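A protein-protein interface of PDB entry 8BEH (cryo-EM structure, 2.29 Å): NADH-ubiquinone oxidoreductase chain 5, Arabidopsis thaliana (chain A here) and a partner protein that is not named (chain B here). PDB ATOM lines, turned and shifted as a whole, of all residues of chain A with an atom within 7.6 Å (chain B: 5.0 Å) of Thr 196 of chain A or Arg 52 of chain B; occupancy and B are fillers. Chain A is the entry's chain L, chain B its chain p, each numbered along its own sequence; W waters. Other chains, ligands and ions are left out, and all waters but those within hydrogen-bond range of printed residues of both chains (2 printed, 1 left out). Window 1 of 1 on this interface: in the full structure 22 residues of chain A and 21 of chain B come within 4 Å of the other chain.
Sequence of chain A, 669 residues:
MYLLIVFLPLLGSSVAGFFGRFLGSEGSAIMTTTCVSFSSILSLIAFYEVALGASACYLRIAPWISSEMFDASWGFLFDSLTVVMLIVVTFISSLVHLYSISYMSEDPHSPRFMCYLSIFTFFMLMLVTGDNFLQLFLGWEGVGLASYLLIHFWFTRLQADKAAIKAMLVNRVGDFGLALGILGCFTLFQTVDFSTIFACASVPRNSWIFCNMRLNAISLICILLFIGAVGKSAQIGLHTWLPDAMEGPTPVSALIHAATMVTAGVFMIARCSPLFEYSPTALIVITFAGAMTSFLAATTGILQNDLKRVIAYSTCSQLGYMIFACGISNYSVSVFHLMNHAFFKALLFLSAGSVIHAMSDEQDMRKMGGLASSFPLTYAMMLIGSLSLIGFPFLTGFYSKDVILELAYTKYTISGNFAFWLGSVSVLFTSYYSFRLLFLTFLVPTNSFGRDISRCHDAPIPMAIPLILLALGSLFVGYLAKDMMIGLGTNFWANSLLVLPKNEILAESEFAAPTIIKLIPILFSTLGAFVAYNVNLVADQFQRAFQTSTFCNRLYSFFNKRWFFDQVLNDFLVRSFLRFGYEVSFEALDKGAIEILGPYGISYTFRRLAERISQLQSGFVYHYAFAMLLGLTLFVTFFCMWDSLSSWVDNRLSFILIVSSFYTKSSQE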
ATOM      1  N   SER A  66      -2.643  -7.351  15.976  1.00  0.00           N
ATOM      2  CA  SER A  66      -1.661  -8.252  15.320  1.00  0.00           C
ATOM      3  C   SER A  66      -0.232  -7.900  15.753  1.00  0.00           C
ATOM      4  O   SER A  66       0.276  -6.894  15.333  1.00  0.00           O
ATOM      5  CB  SER A  66      -1.783  -8.213  13.861  1.00  0.00           C
ATOM      6  OG  SER A  66      -1.342  -9.422  13.299  1.00  0.00           O
ATOM      7  N   GLU A  68       3.219 -10.170  16.015  1.00  0.00           N
ATOM      8  CA  GLU A  68       3.876 -11.501  15.889  1.00  0.00           C
ATOM      9  C   GLU A  68       2.779 -12.575  15.846  1.00  0.00           C
ATOM     10  O   GLU A  68       1.868 -12.447  15.011  1.00  0.00           O
ATOM     11  CB  GLU A  68       4.874 -11.705  17.035  1.00  0.00           C
ATOM     12  CG  GLU A  68       5.931 -12.756  16.764  1.00  0.00           C
ATOM     13  CD  GLU A  68       6.440 -13.472  18.003  1.00  0.00           C
ATOM     14  OE1 GLU A  68       7.490 -13.063  18.532  1.00  0.00           O
ATOM     15  OE2 GLU A  68       5.783 -14.441  18.432  1.00  0.00           O
ATOM     16  N   MET A  69       2.855 -13.587  16.710  1.00  0.00           N
ATOM     17  CA  MET A  69       1.816 -14.666  16.787  1.00  0.00           C
ATOM     18  C   MET A  69       0.452 -14.169  17.313  1.00  0.00           C
ATOM     19  O   MET A  69      -0.518 -14.751  16.901  1.00  0.00           O
ATOM     20  CB  MET A  69       2.270 -15.913  17.556  1.00  0.00           C
ATOM     21  CG  MET A  69       3.476 -16.605  16.978  1.00  0.00           C
ATOM     22  SD  MET A  69       3.222 -17.179  15.296  1.00  0.00           S
ATOM     23  CE  MET A  69       1.960 -18.429  15.529  1.00  0.00           C
ATOM     24  N   PHE A  70       0.384 -13.129  18.145  1.00  0.00           N
ATOM     25  CA  PHE A  70      -0.901 -12.601  18.724  1.00  0.00           C
ATOM     26  C   PHE A  70      -1.803 -12.147  17.565  1.00  0.00           C
ATOM     27  O   PHE A  70      -1.439 -11.285  16.821  1.00  0.00           O
ATOM     28  CB  PHE A  70      -0.620 -11.810  20.010  1.00  0.00           C
ATOM     29  CG  PHE A  70      -1.810 -11.503  20.879  1.00  0.00           C
ATOM     30  CD1 PHE A  70      -2.152 -12.335  21.932  1.00  0.00           C
ATOM     31  CD2 PHE A  70      -2.571 -10.368  20.654  1.00  0.00           C
ATOM     32  CE1 PHE A  70      -3.239 -12.041  22.738  1.00  0.00           C
ATOM     33  CE2 PHE A  70      -3.662 -10.076  21.457  1.00  0.00           C
ATOM     34  CZ  PHE A  70      -3.984 -10.906  22.504  1.00  0.00           C
ATOM     35  N   ASP A  71      -2.995 -12.743  17.446  1.00  0.00           N
ATOM     36  CA  ASP A  71      -3.807 -12.654  16.235  1.00  0.00           C
ATOM     37  C   ASP A  71      -5.254 -12.290  16.537  1.00  0.00           C
ATOM     38  O   ASP A  71      -6.181 -12.812  15.913  1.00  0.00           O
ATOM     39  CB  ASP A  71      -3.752 -13.967  15.455  1.00  0.00           C
ATOM     40  CG  ASP A  71      -4.305 -15.151  16.248  1.00  0.00           C
ATOM     41  OD1 ASP A  71      -4.286 -15.114  17.495  1.00  0.00           O
ATOM     42  OD2 ASP A  71      -4.774 -16.117  15.618  1.00  0.00           O
ATOM     43  N   ALA A  72      -5.484 -11.385  17.482  1.00  0.00           N
ATOM     44  CA  ALA A  72      -6.846 -10.932  17.740  1.00  0.00           C
ATOM     45  C   ALA A  72      -7.394 -10.201  16.519  1.00  0.00           C
ATOM     46  O   ALA A  72      -6.700  -9.394  15.896  1.00  0.00           O
ATOM     47  CB  ALA A  72      -6.882 -10.024  18.966  1.00  0.00           C
ATOM     48  N   ASP A 131     -15.302 -14.733  17.261  1.00  0.00           N
ATOM     49  CA  ASP A 131     -14.621 -15.950  16.841  1.00  0.00           C
ATOM     50  C   ASP A 131     -13.276 -16.139  17.536  1.00  0.00           C
ATOM     51  O   ASP A 131     -12.508 -17.023  17.151  1.00  0.00           O
ATOM     52  CB  ASP A 131     -14.440 -15.954  15.322  1.00  0.00           C
ATOM     53  CG  ASP A 131     -13.400 -14.950  14.847  1.00  0.00           C
ATOM     54  OD1 ASP A 131     -13.097 -13.986  15.577  1.00  0.00           O
ATOM     55  OD2 ASP A 131     -12.882 -15.126  13.728  1.00  0.00           O
ATOM     56  N   PHE A 186      -3.198 -18.044  25.080  1.00  0.00           N
ATOM     57  CA  PHE A 186      -2.264 -17.601  24.053  1.00  0.00           C
ATOM     58  C   PHE A 186      -0.881 -18.196  24.265  1.00  0.00           C
ATOM     59  O   PHE A 186      -0.211 -18.579  23.305  1.00  0.00           O
ATOM     60  CB  PHE A 186      -2.140 -16.083  24.004  1.00  0.00           C
ATOM     61  CG  PHE A 186      -1.117 -15.628  23.015  1.00  0.00           C
ATOM     62  CD1 PHE A 186      -1.321 -15.825  21.657  1.00  0.00           C
ATOM     63  CD2 PHE A 186       0.099 -15.115  23.438  1.00  0.00           C
ATOM     64  CE1 PHE A 186      -0.370 -15.449  20.740  1.00  0.00           C
ATOM     65  CE2 PHE A 186       1.059 -14.739  22.521  1.00  0.00           C
ATOM     66  CZ  PHE A 186       0.827 -14.905  21.171  1.00  0.00           C
ATOM     67  N   PHE A 189      -1.071 -22.058  23.189  1.00  0.00           N
ATOM     68  CA  PHE A 189      -1.376 -22.378  21.800  1.00  0.00           C
ATOM     69  C   PHE A 189      -0.813 -21.376  20.797  1.00  0.00           C
ATOM     70  O   PHE A 189      -0.844 -21.652  19.595  1.00  0.00           O
ATOM     71  CB  PHE A 189      -2.895 -22.494  21.604  1.00  0.00           C
ATOM     72  CG  PHE A 189      -3.542 -23.531  22.480  1.00  0.00           C
ATOM     73  CD1 PHE A 189      -3.477 -24.876  22.150  1.00  0.00           C
ATOM     74  CD2 PHE A 189      -4.212 -23.164  23.634  1.00  0.00           C
ATOM     75  CE1 PHE A 189      -4.070 -25.832  22.953  1.00  0.00           C
ATOM     76  CE2 PHE A 189      -4.809 -24.115  24.441  1.00  0.00           C
ATOM     77  CZ  PHE A 189      -4.734 -25.450  24.102  1.00  0.00           C
ATOM     78  N   GLN A 190      -0.264 -20.247  21.220  1.00  0.00           N
ATOM     79  CA  GLN A 190       0.228 -19.182  20.284  1.00  0.00           C
ATOM     80  C   GLN A 190      -0.930 -18.664  19.427  1.00  0.00           C
ATOM     81  O   GLN A 190      -0.703 -18.279  18.335  1.00  0.00           O
ATOM     82  CB  GLN A 190       1.510 -19.596  19.559  1.00  0.00           C
ATOM     83  CG  GLN A 190       2.701 -19.761  20.497  1.00  0.00           C
ATOM     84  CD  GLN A 190       3.197 -18.479  21.123  1.00  0.00           C
ATOM     85  OE1 GLN A 190       3.733 -17.611  20.453  1.00  0.00           O
ATOM     86  NE2 GLN A 190       3.044 -18.360  22.428  1.00  0.00           N
ATOM     87  N   THR A 191      -2.118 -18.618  19.973  1.00  0.00           N
ATOM     88  CA  THR A 191      -3.242 -18.030  19.262  1.00  0.00           C
ATOM     89  C   THR A 191      -4.347 -17.736  20.264  1.00  0.00           C
ATOM     90  O   THR A 191      -4.369 -18.283  21.367  1.00  0.00           O
ATOM     91  CB  THR A 191      -3.753 -18.949  18.142  1.00  0.00           C
ATOM     92  OG1 THR A 191      -4.791 -18.290  17.411  1.00  0.00           O
ATOM     93  CG2 THR A 191      -4.283 -20.247  18.714  1.00  0.00           C
ATOM     94  N   VAL A 192      -5.263 -16.861  19.863  1.00  0.00           N
ATOM     95  CA  VAL A 192      -6.493 -16.628  20.604  1.00  0.00           C
ATOM     96  C   VAL A 192      -7.723 -16.998  19.784  1.00  0.00           C
ATOM     97  O   VAL A 192      -8.844 -16.774  20.227  1.00  0.00           O
ATOM     98  CB  VAL A 192      -6.581 -15.171  21.102  1.00  0.00           C
ATOM     99  CG1 VAL A 192      -5.501 -14.902  22.138  1.00  0.00           C
ATOM    100  CG2 VAL A 192      -6.481 -14.200  19.942  1.00  0.00           C
ATOM    101  N   ASP A 193      -7.524 -17.490  18.566  1.00  0.00           N
ATOM    102  CA  ASP A 193      -8.631 -17.977  17.684  1.00  0.00           C
ATOM    103  C   ASP A 193      -9.333 -19.231  18.245  1.00  0.00           C
ATOM    104  O   ASP A 193      -8.700 -20.199  18.479  1.00  0.00           O
ATOM    105  CB  ASP A 193      -8.152 -18.235  16.261  1.00  0.00           C
ATOM    106  CG  ASP A 193      -9.207 -18.685  15.290  1.00  0.00           C
ATOM    107  OD1 ASP A 193      -9.817 -17.814  14.686  1.00  0.00           O
ATOM    108  OD2 ASP A 193      -9.398 -19.898  15.155  1.00  0.00           O
ATOM    109  N   PHE A 194     -10.644 -19.187  18.285  1.00  0.00           N
ATOM    110  CA  PHE A 194     -11.396 -20.299  18.867  1.00  0.00           C
ATOM    111  C   PHE A 194     -11.180 -21.594  18.089  1.00  0.00           C
ATOM    112  O   PHE A 194     -10.914 -22.644  18.683  1.00  0.00           O
ATOM    113  CB  PHE A 194     -12.883 -19.950  18.928  1.00  0.00           C
ATOM    114  CG  PHE A 194     -13.253 -19.071  20.088  1.00  0.00           C
ATOM    115  CD1 PHE A 194     -12.548 -19.137  21.282  1.00  0.00           C
ATOM    116  CD2 PHE A 194     -14.294 -18.164  19.981  1.00  0.00           C
ATOM    117  CE1 PHE A 194     -12.884 -18.318  22.350  1.00  0.00           C
ATOM    118  CE2 PHE A 194     -14.631 -17.347  21.042  1.00  0.00           C
ATOM    119  CZ  PHE A 194     -13.925 -17.425  22.227  1.00  0.00           C
ATOM    120  N   SER A 195     -11.265 -21.521  16.764  1.00  0.00           N
ATOM    121  CA  SER A 195     -11.185 -22.720  15.867  1.00  0.00           C
ATOM    122  C   SER A 195      -9.832 -23.415  16.011  1.00  0.00           C
ATOM    123  O   SER A 195      -9.831 -24.610  16.177  1.00  0.00           O
ATOM    124  CB  SER A 195     -11.568 -22.452  14.389  1.00  0.00           C
ATOM    125  OG  SER A 195     -12.663 -21.601  14.252  1.00  0.00           O
ATOM    126  N   THR A 196      -8.756 -22.618  16.056  1.00  0.00           N
ATOM    127  CA  THR A 196      -7.405 -23.165  16.183  1.00  0.00           C
ATOM    128  C   THR A 196      -7.227 -23.803  17.563  1.00  0.00           C
ATOM    129  O   THR A 196      -6.766 -24.917  17.620  1.00  0.00           O
ATOM    130  CB  THR A 196      -6.356 -22.154  15.669  1.00  0.00           C
ATOM    131  OG1 THR A 196      -6.685 -21.720  14.352  1.00  0.00           O
ATOM    132  CG2 THR A 196      -4.946 -22.695  15.750  1.00  0.00           C
ATOM    133  N   ILE A 197      -7.658 -23.119  18.606  1.00  0.00           N
ATOM    134  CA  ILE A 197      -7.494 -23.631  19.962  1.00  0.00           C
ATOM    135  C   ILE A 197      -8.264 -24.934  20.139  1.00  0.00           C
ATOM    136  O   ILE A 197      -7.745 -25.906  20.699  1.00  0.00           O
ATOM    137  CB  ILE A 197      -7.926 -22.571  20.994  1.00  0.00           C
ATOM    138  CG1 ILE A 197      -6.901 -21.435  21.057  1.00  0.00           C
ATOM    139  CG2 ILE A 197      -8.112 -23.202  22.373  1.00  0.00           C
ATOM    140  CD1 ILE A 197      -7.429 -20.169  21.695  1.00  0.00           C
ATOM    141  N   PHE A 198      -9.507 -24.980  19.653  1.00  0.00           N
ATOM    142  CA  PHE A 198     -10.308 -26.189  19.811  1.00  0.00           C
ATOM    143  C   PHE A 198      -9.756 -27.342  18.985  1.00  0.00           C
ATOM    144  O   PHE A 198      -9.870 -28.501  19.393  1.00  0.00           O
ATOM    145  CB  PHE A 198     -11.770 -25.920  19.451  1.00  0.00           C
ATOM    146  CG  PHE A 198     -12.407 -24.840  20.277  1.00  0.00           C
ATOM    147  CD1 PHE A 198     -11.951 -24.572  21.563  1.00  0.00           C
ATOM    148  CD2 PHE A 198     -13.469 -24.107  19.784  1.00  0.00           C
ATOM    149  CE1 PHE A 198     -12.528 -23.578  22.321  1.00  0.00           C
ATOM    150  CE2 PHE A 198     -14.051 -23.117  20.539  1.00  0.00           C
ATOM    151  CZ  PHE A 198     -13.581 -22.852  21.813  1.00  0.00           C
ATOM    152  N   ALA A 199      -9.150 -27.049  17.835  1.00  0.00           N
ATOM    153  CA  ALA A 199      -8.518 -28.098  17.047  1.00  0.00           C
ATOM    154  C   ALA A 199      -7.263 -28.651  17.710  1.00  0.00           C
ATOM    155  O   ALA A 199      -6.888 -29.795  17.437  1.00  0.00           O
ATOM    156  CB  ALA A 199      -8.184 -27.575  15.654  1.00  0.00           C
ATOM    157  N   CYS A 200      -6.617 -27.880  18.584  1.00  0.00           N
ATOM    158  CA  CYS A 200      -5.345 -28.269  19.173  1.00  0.00           C
ATOM    159  C   CYS A 200      -5.463 -28.775  20.605  1.00  0.00           C
ATOM    160  O   CYS A 200      -4.501 -29.354  21.114  1.00  0.00           O
ATOM    161  CB  CYS A 200      -4.367 -27.083  19.154  1.00  0.00           C
ATOM    162  SG  CYS A 200      -3.788 -26.563  17.532  1.00  0.00           S
ATOM    163  N   ALA A 201      -6.617 -28.592  21.254  1.00  0.00           N
ATOM    164  CA  ALA A 201      -6.691 -28.664  22.710  1.00  0.00           C
ATOM    165  C   ALA A 201      -6.404 -30.050  23.273  1.00  0.00           C
ATOM    166  O   ALA A 201      -6.031 -30.160  24.443  1.00  0.00           O
ATOM    167  CB  ALA A 201      -8.064 -28.194  23.188  1.00  0.00           C
ATOM    168  N   ALA B  48       4.390 -20.362  10.704  1.00  0.00           N
ATOM    169  CA  ALA B  48       3.423 -20.787  11.719  1.00  0.00           C
ATOM    170  C   ALA B  48       2.017 -20.151  11.481  1.00  0.00           C
ATOM    171  O   ALA B  48       1.061 -20.848  11.659  1.00  0.00           O
ATOM    172  CB  ALA B  48       3.982 -20.624  13.120  1.00  0.00           C
ATOM    173  N   LYS B  49       1.929 -18.926  10.981  1.00  0.00           N
ATOM    174  CA  LYS B  49       0.643 -18.235  10.742  1.00  0.00           C
ATOM    175  C   LYS B  49      -0.082 -18.885   9.557  1.00  0.00           C
ATOM    176  O   LYS B  49      -1.287 -18.989   9.610  1.00  0.00           O
ATOM    177  CB  LYS B  49       0.837 -16.721  10.607  1.00  0.00           C
ATOM    178  CG  LYS B  49       1.555 -16.066  11.771  1.00  0.00           C
ATOM    179  CD  LYS B  49       0.803 -14.956  12.428  1.00  0.00           C
ATOM    180  CE  LYS B  49       0.320 -13.880  11.488  1.00  0.00           C
ATOM    181  NZ  LYS B  49       1.436 -13.237  10.773  1.00  0.00           N
ATOM    182  N   ILE B  50       0.675 -19.237   8.539  1.00  0.00           N
ATOM    183  CA  ILE B  50       0.124 -19.955   7.369  1.00  0.00           C
ATOM    184  C   ILE B  50      -0.399 -21.348   7.804  1.00  0.00           C
ATOM    185  O   ILE B  50      -1.536 -21.612   7.474  1.00  0.00           O
ATOM    186  CB  ILE B  50       1.126 -19.959   6.198  1.00  0.00           C
ATOM    187  CG1 ILE B  50       1.276 -18.577   5.568  1.00  0.00           C
ATOM    188  CG2 ILE B  50       0.764 -21.000   5.147  1.00  0.00           C
ATOM    189  CD1 ILE B  50       2.601 -18.355   4.915  1.00  0.00           C
ATOM    190  N   LEU B  51       0.352 -22.096   8.599  1.00  0.00           N
ATOM    191  CA  LEU B  51      -0.096 -23.393   9.109  1.00  0.00           C
ATOM    192  C   LEU B  51      -1.333 -23.243   9.990  1.00  0.00           C
ATOM    193  O   LEU B  51      -2.245 -24.080   9.947  1.00  0.00           O
ATOM    194  CB  LEU B  51       1.032 -24.076   9.880  1.00  0.00           C
ATOM    195  CG  LEU B  51       2.203 -24.622   9.060  1.00  0.00           C
ATOM    196  CD1 LEU B  51       3.246 -25.261   9.962  1.00  0.00           C
ATOM    197  CD2 LEU B  51       1.730 -25.599   7.998  1.00  0.00           C
ATOM    198  N   ARG B  52      -1.482 -22.154  10.742  1.00  0.00           N
ATOM    199  CA  ARG B  52      -2.669 -21.883  11.587  1.00  0.00           C
ATOM    200  C   ARG B  52      -3.946 -21.717  10.709  1.00  0.00           C
ATOM    201  O   ARG B  52      -4.955 -22.239  11.120  1.00  0.00           O
ATOM    202  CB  ARG B  52      -2.377 -20.740  12.570  1.00  0.00           C
ATOM    203  CG  ARG B  52      -3.506 -20.333  13.496  1.00  0.00           C
ATOM    204  CD  ARG B  52      -2.932 -19.409  14.543  1.00  0.00           C
ATOM    205  NE  ARG B  52      -2.613 -18.099  14.014  1.00  0.00           N
ATOM    206  CZ  ARG B  52      -1.893 -17.194  14.646  1.00  0.00           C
ATOM    207  NH1 ARG B  52      -1.390 -17.467  15.831  1.00  0.00           N
ATOM    208  NH2 ARG B  52      -1.676 -16.026  14.092  1.00  0.00           N
ATOM    209  N   GLU B  53      -3.876 -21.001   9.618  1.00  0.00           N
ATOM    210  CA  GLU B  53      -4.991 -20.858   8.633  1.00  0.00           C
ATOM    211  C   GLU B  53      -5.492 -22.268   8.160  1.00  0.00           C
ATOM    212  O   GLU B  53      -6.674 -22.447   8.222  1.00  0.00           O
ATOM    213  CB  GLU B  53      -4.584 -19.869   7.529  1.00  0.00           C
ATOM    214  CG  GLU B  53      -5.652 -18.865   7.228  1.00  0.00           C
ATOM    215  CD  GLU B  53      -6.094 -18.076   8.443  1.00  0.00           C
ATOM    216  OE1 GLU B  53      -5.233 -17.697   9.244  1.00  0.00           O
ATOM    217  OE2 GLU B  53      -7.302 -17.872   8.590  1.00  0.00           O
ATOM    218  N   LYS B  54      -4.586 -23.223   7.909  1.00  0.00           N
ATOM    219  CA  LYS B  54      -4.945 -24.656   7.558  1.00  0.00           C
ATOM    220  C   LYS B  54      -5.783 -25.331   8.646  1.00  0.00           C
ATOM    221  O   LYS B  54      -6.851 -25.718   8.328  1.00  0.00           O
ATOM    222  CB  LYS B  54      -3.678 -25.419   7.150  1.00  0.00           C
ATOM    223  CG  LYS B  54      -2.956 -24.845   5.937  1.00  0.00           C
ATOM    224  CD  LYS B  54      -1.783 -25.681   5.480  1.00  0.00           C
ATOM    225  CE  LYS B  54      -0.718 -24.929   4.716  1.00  0.00           C
ATOM    226  NZ  LYS B  54      -1.246 -24.146   3.577  1.00  0.00           N
ATOM    227  N   VAL B  55      -5.344 -25.242   9.905  1.00  0.00           N
ATOM    228  CA  VAL B  55      -6.057 -25.799  11.068  1.00  0.00           C
ATOM    229  C   VAL B  55      -7.401 -25.127  11.182  1.00  0.00           C
ATOM    230  O   VAL B  55      -8.345 -25.880  11.264  1.00  0.00           O
ATOM    231  CB  VAL B  55      -5.209 -25.751  12.363  1.00  0.00           C
ATOM    232  CG1 VAL B  55      -5.969 -26.154  13.600  1.00  0.00           C
ATOM    233  CG2 VAL B  55      -3.920 -26.538  12.218  1.00  0.00           C
ATOM    234  N   LYS B  56      -7.434 -23.786  11.146  1.00  0.00           N
ATOM    235  CA  LYS B  56      -8.660 -23.015  11.288  1.00  0.00           C
ATOM    236  C   LYS B  56      -9.706 -23.624  10.322  1.00  0.00           C
ATOM    237  O   LYS B  56     -10.729 -24.060  10.800  1.00  0.00           O
ATOM    238  CB  LYS B  56      -8.416 -21.512  11.041  1.00  0.00           C
ATOM    239  CG  LYS B  56      -9.578 -20.563  11.251  1.00  0.00           C
ATOM    240  CD  LYS B  56      -9.257 -19.119  10.917  1.00  0.00           C
ATOM    241  CE  LYS B  56      -8.319 -18.433  11.889  1.00  0.00           C
ATOM    242  NZ  LYS B  56      -6.891 -18.490  11.492  1.00  0.00           N
ATOM    243  N   TYR B  77       1.413 -27.507  12.886  1.00  0.00           N
ATOM    244  CA  TYR B  77       1.290 -26.188  13.495  1.00  0.00           C
ATOM    245  C   TYR B  77       1.936 -26.150  14.872  1.00  0.00           C
ATOM    246  O   TYR B  77       2.660 -25.206  15.198  1.00  0.00           O
ATOM    247  CB  TYR B  77      -0.175 -25.768  13.599  1.00  0.00           C
ATOM    248  CG  TYR B  77      -0.355 -24.551  14.479  1.00  0.00           C
ATOM    249  CD1 TYR B  77       0.074 -23.300  14.052  1.00  0.00           C
ATOM    250  CD2 TYR B  77      -0.910 -24.655  15.747  1.00  0.00           C
ATOM    251  CE1 TYR B  77      -0.068 -22.191  14.846  1.00  0.00           C
ATOM    252  CE2 TYR B  77      -1.054 -23.546  16.553  1.00  0.00           C
ATOM    253  CZ  TYR B  77      -0.629 -22.311  16.093  1.00  0.00           C
ATOM    254  OH  TYR B  77      -0.762 -21.193  16.876  1.00  0.00           O
HETATM  255  O   HOH W   1      -5.649 -16.741  13.400  1.00  0.00           O
HETATM  256  O   HOH W   2       2.441 -11.710  12.570  1.00  0.00           O
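Among the printed residues, merely in contact across the chains: Glu 68 of chain A with Lys 49 of chain B, Met 69 of chain A with Ala 48 of chain B, Thr 191 of chain A with Arg 52 of chain B, Thr 191 of chain A with Tyr 77 of chain B, Asp 193 of chain A with Lys 56 of chain B, Thr 196 of chain A with Arg 52 of chain B, Thr 196 of chain A with Lys 56 of chain B, Ala 199 of chain A with Val 55 of chain B and Cys 200 of chain A with Tyr 77 of chain B.
The backbone carbonyl oxygen (O) of Gln 190 of chain A sits at hydrogen-bond distance from the guanidinium group (NH1) of Arg 52 of chain B.
The backbone carbonyl oxygen (O) of Met 69 of chain A sits at hydrogen-bond distance from the guanidinium group (NH1) of Arg 52 of chain B, 3.0 Å away.
OD2 of Asp 71 of chain A is in salt-bridge range of NE of Arg 52 of chain B (3.3 Å).
The backbone carbonyl oxygen of Phe 189 of chain A lies within hydrogen-bond range of the side-chain hydroxyl of Tyr 77 of chain B (2.8 Å).
The backbone carbonyl oxygen of Gln 190 of chain A is in hydrogen-bond range of the side-chain hydroxyl of Tyr 77 of chain B, at 3.3 Å.
Of chain B, only Arg 52 and Lys 56 come within 4 Å of Thr 196 of chain A.
Arg 52 of chain B touches just these residues of chain A: Met 69, Asp 71, Gln 190, Thr 191 and Thr 196.
Of the printed residues of chain B, Cys 200 of chain A touches Tyr 77.
Printed residues of chain A within 4 Å of Ala 48 of chain B: Met 69 (3.8 Å).
Printed residues of chain B within 4 Å of Asp 71 of chain A: Arg 52.
Of the printed residues of chain B, Ala 199 of chain A touches Val 55.
Phe 194 of chain A touches none of the printed residues of chain B.
Ser 66 of chain A touches none of the printed residues of chain B.
The nearest residue of chain B that does not touch Thr 196 of chain A is Tyr 77 of chain B (4.1 Å).
The nearest printed residue of chain A that does not touch Ala 48 of chain B is Gln 190 of chain A (7.0 Å).
OG1 of Thr 191 of chain A sits at hydrogen-bond distance from OD2 of Asp 71 of chain A, 2.8 Å away.
The backbone NH (N) of Ser 195 of chain A is in hydrogen-bond range of the side-chain carboxylate (OD2) of Asp 193 of chain A (3.0 Å).
OD1 of Asp 71 of chain A is in hydrogen-bond range of N of Val 192 of chain A (3.1 Å).
The backbone carbonyl oxygen (O) of Phe 186 of chain A sits close to the side-chain amide nitrogen (NE2) of Gln 190 of chain A (3.4 Å).
The side-chain amino group (NZ) of Lys 56 of chain B is in salt-bridge range of the side-chain carboxylate (OE1) of Glu 53 of chain B (2.9 Å).
The backbone carbonyl oxygen (O) of Thr 196 of chain A is in hydrogen-bond range of the side-chain sulfur (SG) of Cys 200 of chain A, 3.4 Å away.
Of the 10 printed residues of chain B, 6 touch a printed residue of chain A.
Along chain B the printed residues that touch a printed residue of chain A span positions 48 to 77.
Among the printed residues, 14 pairs touch across the chains.
Among the printed residues, Asp or Glu carboxylates within 4 Å of a Lys or Arg side-chain nitrogen of the other chain: Asp 71 of chain A with Arg 52 of chain B (3.3 Å).
Water W1 lies within hydrogen-bond range of OD2 of Asp 71 of chain A (2.5 Å), NZ of Lys 56 of chain B (2.9 Å) and NE of Arg 52 of chain B (3.4 Å).
Water W2 lies within hydrogen-bond range of NZ of Lys 49 of chain B and O of Glu 68 of chain A.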
